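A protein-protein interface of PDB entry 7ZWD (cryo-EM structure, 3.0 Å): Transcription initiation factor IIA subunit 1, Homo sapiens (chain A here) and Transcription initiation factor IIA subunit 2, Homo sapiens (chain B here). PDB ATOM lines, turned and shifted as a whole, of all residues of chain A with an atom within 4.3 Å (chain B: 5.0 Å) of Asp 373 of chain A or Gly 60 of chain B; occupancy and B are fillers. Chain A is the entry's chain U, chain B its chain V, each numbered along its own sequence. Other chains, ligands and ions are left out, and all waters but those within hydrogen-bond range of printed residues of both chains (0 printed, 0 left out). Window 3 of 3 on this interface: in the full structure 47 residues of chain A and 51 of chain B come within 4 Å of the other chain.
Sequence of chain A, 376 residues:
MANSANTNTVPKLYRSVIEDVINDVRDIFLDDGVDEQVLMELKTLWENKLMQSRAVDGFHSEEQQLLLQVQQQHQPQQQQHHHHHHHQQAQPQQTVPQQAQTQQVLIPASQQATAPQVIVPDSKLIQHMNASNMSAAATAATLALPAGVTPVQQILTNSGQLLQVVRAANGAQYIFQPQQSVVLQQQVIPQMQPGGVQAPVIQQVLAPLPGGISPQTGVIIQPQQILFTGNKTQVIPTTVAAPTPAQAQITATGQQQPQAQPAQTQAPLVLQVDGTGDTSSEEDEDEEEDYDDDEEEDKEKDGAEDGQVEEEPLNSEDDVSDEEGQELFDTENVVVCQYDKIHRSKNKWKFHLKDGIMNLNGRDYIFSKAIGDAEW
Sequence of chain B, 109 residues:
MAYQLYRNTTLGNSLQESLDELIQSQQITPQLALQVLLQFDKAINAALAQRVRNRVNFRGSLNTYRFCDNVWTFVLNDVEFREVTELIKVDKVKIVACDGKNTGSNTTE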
ATOM      1  N   LYS A 348       4.444 -25.171  20.978  1.00  0.00           N
ATOM      2  CA  LYS A 348       4.784 -24.903  22.363  1.00  0.00           C
ATOM      3  C   LYS A 348       6.102 -25.582  22.693  1.00  0.00           C
ATOM      4  O   LYS A 348       6.210 -26.805  22.604  1.00  0.00           O
ATOM      5  CB  LYS A 348       3.682 -25.402  23.291  1.00  0.00           C
ATOM      6  CG  LYS A 348       2.558 -24.419  23.521  1.00  0.00           C
ATOM      7  CD  LYS A 348       2.825 -23.582  24.760  1.00  0.00           C
ATOM      8  CE  LYS A 348       1.621 -22.731  25.120  1.00  0.00           C
ATOM      9  NZ  LYS A 348       1.772 -22.088  26.454  1.00  0.00           N
ATOM     10  N   TRP A 349       7.091 -24.790  23.075  1.00  0.00           N
ATOM     11  CA  TRP A 349       8.370 -25.292  23.539  1.00  0.00           C
ATOM     12  C   TRP A 349       8.366 -25.351  25.054  1.00  0.00           C
ATOM     13  O   TRP A 349       7.854 -24.441  25.710  1.00  0.00           O
ATOM     14  CB  TRP A 349       9.502 -24.395  23.061  1.00  0.00           C
ATOM     15  CG  TRP A 349       9.673 -24.411  21.615  1.00  0.00           C
ATOM     16  CD1 TRP A 349       8.862 -23.846  20.693  1.00  0.00           C
ATOM     17  CD2 TRP A 349      10.731 -25.031  20.899  1.00  0.00           C
ATOM     18  NE1 TRP A 349       9.350 -24.070  19.436  1.00  0.00           N
ATOM     19  CE2 TRP A 349      10.501 -24.800  19.538  1.00  0.00           C
ATOM     20  CE3 TRP A 349      11.854 -25.758  21.278  1.00  0.00           C
ATOM     21  CZ2 TRP A 349      11.349 -25.268  18.559  1.00  0.00           C
ATOM     22  CZ3 TRP A 349      12.688 -26.220  20.309  1.00  0.00           C
ATOM     23  CH2 TRP A 349      12.436 -25.978  18.963  1.00  0.00           C
ATOM     24  N   LYS A 350       8.936 -26.412  25.603  1.00  0.00           N
ATOM     25  CA  LYS A 350       9.063 -26.590  27.038  1.00  0.00           C
ATOM     26  C   LYS A 350      10.509 -26.934  27.338  1.00  0.00           C
ATOM     27  O   LYS A 350      10.985 -28.005  26.951  1.00  0.00           O
ATOM     28  CB  LYS A 350       8.132 -27.692  27.531  1.00  0.00           C
ATOM     29  CG  LYS A 350       8.108 -27.859  29.026  1.00  0.00           C
ATOM     30  CD  LYS A 350       7.076 -26.949  29.648  1.00  0.00           C
ATOM     31  CE  LYS A 350       6.981 -27.155  31.146  1.00  0.00           C
ATOM     32  NZ  LYS A 350       6.080 -26.155  31.778  1.00  0.00           N
ATOM     33  N   PHE A 351      11.206 -26.033  28.016  1.00  0.00           N
ATOM     34  CA  PHE A 351      12.617 -26.202  28.314  1.00  0.00           C
ATOM     35  C   PHE A 351      12.770 -26.637  29.758  1.00  0.00           C
ATOM     36  O   PHE A 351      12.323 -25.932  30.664  1.00  0.00           O
ATOM     37  CB  PHE A 351      13.385 -24.901  28.113  1.00  0.00           C
ATOM     38  CG  PHE A 351      12.915 -24.090  26.960  1.00  0.00           C
ATOM     39  CD1 PHE A 351      13.345 -24.352  25.694  1.00  0.00           C
ATOM     40  CD2 PHE A 351      12.050 -23.047  27.156  1.00  0.00           C
ATOM     41  CE1 PHE A 351      12.912 -23.595  24.652  1.00  0.00           C
ATOM     42  CE2 PHE A 351      11.617 -22.295  26.112  1.00  0.00           C
ATOM     43  CZ  PHE A 351      12.046 -22.568  24.863  1.00  0.00           C
ATOM     44  N   GLY A 372      11.054 -23.580  31.807  1.00  0.00           N
ATOM     45  CA  GLY A 372      10.451 -22.491  31.083  1.00  0.00           C
ATOM     46  C   GLY A 372       9.540 -22.997  29.985  1.00  0.00           C
ATOM     47  O   GLY A 372       9.642 -24.129  29.530  1.00  0.00           O
ATOM     48  N   ASP A 373       8.646 -22.121  29.564  1.00  0.00           N
ATOM     49  CA  ASP A 373       7.726 -22.404  28.483  1.00  0.00           C
ATOM     50  C   ASP A 373       7.796 -21.271  27.475  1.00  0.00           C
ATOM     51  O   ASP A 373       8.144 -20.142  27.815  1.00  0.00           O
ATOM     52  CB  ASP A 373       6.306 -22.569  29.002  1.00  0.00           C
ATOM     53  CG  ASP A 373       5.342 -23.007  27.926  1.00  0.00           C
ATOM     54  OD1 ASP A 373       5.151 -22.251  26.954  1.00  0.00           O
ATOM     55  OD2 ASP A 373       4.771 -24.111  28.047  1.00  0.00           O
ATOM     56  N   ALA A 374       7.469 -21.582  26.228  1.00  0.00           N
ATOM     57  CA  ALA A 374       7.472 -20.563  25.197  1.00  0.00           C
ATOM     58  C   ALA A 374       6.558 -21.008  24.075  1.00  0.00           C
ATOM     59  O   ALA A 374       6.257 -22.189  23.934  1.00  0.00           O
ATOM     60  CB  ALA A 374       8.878 -20.303  24.666  1.00  0.00           C
ATOM     61  N   GLU A 375       6.110 -20.052  23.276  1.00  0.00           N
ATOM     62  CA  GLU A 375       5.299 -20.347  22.108  1.00  0.00           C
ATOM     63  C   GLU A 375       5.919 -19.675  20.898  1.00  0.00           C
ATOM     64  O   GLU A 375       5.964 -18.445  20.820  1.00  0.00           O
ATOM     65  CB  GLU A 375       3.858 -19.882  22.286  1.00  0.00           C
ATOM     66  CG  GLU A 375       2.984 -20.255  21.104  1.00  0.00           C
ATOM     67  CD  GLU A 375       1.538 -19.857  21.286  1.00  0.00           C
ATOM     68  OE1 GLU A 375       1.208 -19.278  22.341  1.00  0.00           O
ATOM     69  OE2 GLU A 375       0.733 -20.122  20.369  1.00  0.00           O
ATOM     70  N   PHE B  58      10.408 -19.505  33.671  1.00  0.00           N
ATOM     71  CA  PHE B  58      10.235 -18.377  32.781  1.00  0.00           C
ATOM     72  C   PHE B  58       9.157 -18.674  31.759  1.00  0.00           C
ATOM     73  O   PHE B  58       8.882 -19.825  31.430  1.00  0.00           O
ATOM     74  CB  PHE B  58      11.535 -17.988  32.084  1.00  0.00           C
ATOM     75  CG  PHE B  58      12.181 -19.095  31.328  1.00  0.00           C
ATOM     76  CD1 PHE B  58      13.078 -19.932  31.943  1.00  0.00           C
ATOM     77  CD2 PHE B  58      11.920 -19.274  29.990  1.00  0.00           C
ATOM     78  CE1 PHE B  58      13.680 -20.935  31.248  1.00  0.00           C
ATOM     79  CE2 PHE B  58      12.522 -20.274  29.295  1.00  0.00           C
ATOM     80  CZ  PHE B  58      13.402 -21.106  29.924  1.00  0.00           C
ATOM     81  N   ARG B  59       8.521 -17.611  31.302  1.00  0.00           N
ATOM     82  CA  ARG B  59       7.576 -17.674  30.202  1.00  0.00           C
ATOM     83  C   ARG B  59       7.891 -16.561  29.229  1.00  0.00           C
ATOM     84  O   ARG B  59       8.109 -15.419  29.634  1.00  0.00           O
ATOM     85  CB  ARG B  59       6.144 -17.534  30.674  1.00  0.00           C
ATOM     86  CG  ARG B  59       5.546 -18.787  31.233  1.00  0.00           C
ATOM     87  CD  ARG B  59       4.085 -18.844  30.874  1.00  0.00           C
ATOM     88  NE  ARG B  59       3.263 -19.235  32.008  1.00  0.00           N
ATOM     89  CZ  ARG B  59       1.939 -19.280  31.979  1.00  0.00           C
ATOM     90  NH1 ARG B  59       1.289 -18.955  30.871  1.00  0.00           N
ATOM     91  NH2 ARG B  59       1.265 -19.647  33.057  1.00  0.00           N
ATOM     92  N   GLY B  60       7.910 -16.889  27.946  1.00  0.00           N
ATOM     93  CA  GLY B  60       8.182 -15.894  26.937  1.00  0.00           C
ATOM     94  C   GLY B  60       7.619 -16.353  25.617  1.00  0.00           C
ATOM     95  O   GLY B  60       6.958 -17.385  25.530  1.00  0.00           O
ATOM     96  N   SER B  61       7.874 -15.571  24.591  1.00  0.00           N
ATOM     97  CA  SER B  61       7.519 -15.932  23.229  1.00  0.00           C
ATOM     98  C   SER B  61       8.820 -16.201  22.496  1.00  0.00           C
ATOM     99  O   SER B  61       9.510 -15.266  22.089  1.00  0.00           O
ATOM    100  CB  SER B  61       6.720 -14.826  22.556  1.00  0.00           C
ATOM    101  OG  SER B  61       7.588 -13.894  21.945  1.00  0.00           O
ATOM    102  N   LEU B  62       9.153 -17.474  22.339  1.00  0.00           N
ATOM    103  CA  LEU B  62      10.387 -17.857  21.672  1.00  0.00           C
ATOM    104  C   LEU B  62      10.465 -17.205  20.307  1.00  0.00           C
ATOM    105  O   LEU B  62       9.671 -17.513  19.420  1.00  0.00           O
ATOM    106  CB  LEU B  62      10.444 -19.371  21.533  1.00  0.00           C
ATOM    107  CG  LEU B  62      11.627 -19.945  20.779  1.00  0.00           C
ATOM    108  CD1 LEU B  62      12.793 -20.094  21.697  1.00  0.00           C
ATOM    109  CD2 LEU B  62      11.244 -21.268  20.205  1.00  0.00           C
ATOM    110  N   LEU B  76      14.455 -15.443  23.016  1.00  0.00           N
ATOM    111  CA  LEU B  76      13.100 -15.247  23.492  1.00  0.00           C
ATOM    112  C   LEU B  76      12.832 -13.763  23.671  1.00  0.00           C
ATOM    113  O   LEU B  76      13.734 -12.995  24.001  1.00  0.00           O
ATOM    114  CB  LEU B  76      12.868 -15.969  24.814  1.00  0.00           C
ATOM    115  CG  LEU B  76      12.908 -17.487  24.859  1.00  0.00           C
ATOM    116  CD1 LEU B  76      14.298 -17.957  25.104  1.00  0.00           C
ATOM    117  CD2 LEU B  76      12.017 -17.970  25.955  1.00  0.00           C
ATOM    118  N   ASN B  77      11.584 -13.367  23.458  1.00  0.00           N
ATOM    119  CA  ASN B  77      11.180 -11.975  23.531  1.00  0.00           C
ATOM    120  C   ASN B  77      10.094 -11.798  24.577  1.00  0.00           C
ATOM    121  O   ASN B  77       9.214 -12.648  24.725  1.00  0.00           O
ATOM    122  CB  ASN B  77      10.667 -11.484  22.189  1.00  0.00           C
ATOM    123  CG  ASN B  77      11.766 -11.309  21.189  1.00  0.00           C
ATOM    124  OD1 ASN B  77      12.922 -11.596  21.473  1.00  0.00           O
ATOM    125  ND2 ASN B  77      11.419 -10.835  20.005  1.00  0.00           N
ATOM    126  N   ASP B  78      10.153 -10.675  25.286  1.00  0.00           N
ATOM    127  CA  ASP B  78       9.163 -10.315  26.298  1.00  0.00           C
ATOM    128  C   ASP B  78       8.958 -11.457  27.288  1.00  0.00           C
ATOM    129  O   ASP B  78       7.875 -12.021  27.426  1.00  0.00           O
ATOM    130  CB  ASP B  78       7.846  -9.901  25.644  1.00  0.00           C
ATOM    131  CG  ASP B  78       7.935  -8.548  24.967  1.00  0.00           C
ATOM    132  OD1 ASP B  78       8.158  -8.504  23.740  1.00  0.00           O
ATOM    133  OD2 ASP B  78       7.784  -7.523  25.665  1.00  0.00           O
ATOM    134  N   VAL B  79      10.032 -11.780  27.980  1.00  0.00           N
ATOM    135  CA  VAL B  79      10.088 -12.925  28.874  1.00  0.00           C
ATOM    136  C   VAL B  79       9.942 -12.446  30.305  1.00  0.00           C
ATOM    137  O   VAL B  79      10.350 -11.331  30.646  1.00  0.00           O
ATOM    138  CB  VAL B  79      11.409 -13.682  28.683  1.00  0.00           C
ATOM    139  CG1 VAL B  79      11.360 -15.034  29.354  1.00  0.00           C
ATOM    140  CG2 VAL B  79      11.690 -13.816  27.223  1.00  0.00           C
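The side-chain amino group (NZ) of Lys 348 of chain A is in salt-bridge range of the side-chain carboxylate (OD1) of Asp 373 of chain A, 3.4 Å away.
The backbone NH (N) of Trp 349 of chain A sits at hydrogen-bond distance from the backbone carbonyl oxygen (O) of Ala 374 of chain A (2.9 Å).
The backbone NH (N) of Phe 351 of chain A is in hydrogen-bond range of the backbone carbonyl oxygen (O) of Gly 372 of chain A, at 2.9 Å.
The backbone carbonyl oxygen of Ser 61 of chain B lies within hydrogen-bond range of the backbone NH of Asn 77 of chain B (3.1 Å).
N of Asp 373 of chain A is in hydrogen-bond range of O of Phe 58 of chain B (3.0 Å).
The backbone carbonyl oxygen of Asp 373 of chain A lies within hydrogen-bond range of the backbone NH of Gly 60 of chain B (3.3 Å).
Of chain B, only Phe 58 (3.0 Å), Arg 59 (3.5 Å) and Gly 60 (3.3 Å) come within 4 Å of Asp 373 of chain A.
Of the printed residues of chain A, Gly 60 of chain B touches Asp 373, Ala 374 and Glu 375.
Of the printed residues of chain A, Leu 62 of chain B touches Trp 349, Ala 374 and Glu 375.
Of the printed residues of chain B, Trp 349 of chain A touches Leu 62.
Of the printed residues of chain A, Phe 58 of chain B touches Phe 351, Gly 372 and Asp 373.
Of the printed residues of chain A, Ser 61 of chain B touches Glu 375 (3.8 Å).
The nearest residue of chain B that does not touch Asp 373 of chain A is Leu 76 of chain B (4.8 Å).
The nearest printed residue of chain A that does not touch Gly 60 of chain B is Gly 372 of chain A (6.6 Å).
Of the 8 printed residues of chain A, 6 touch a printed residue of chain B.
Hydrophobic or aromatic side chains of chain A that line the printed part of chain B: Trp 349, Phe 351 and Ala 374.
Among the printed residues, no Asp or Glu carboxylate lies within 4 Å of a Lys or Arg side-chain nitrogen of the other chain.
Among the printed residues, pairs that only touch across the chains: Gly 372 of chain A with Phe 58 of chain B, Ala 374 of chain A with Gly 60 of chain B, Trp 349 of chain A with Leu 62 of chain B, Asp 373 of chain A with Arg 59 of chain B, Phe 351 of chain A with Phe 58 of chain B, Glu 375 of chain A with Gly 60 of chain B, Ala 374 of chain A with Leu 62 of chain B, Glu 375 of chain A with Leu 62 of chain B and Glu 375 of chain A with Ser 61 of chain B.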
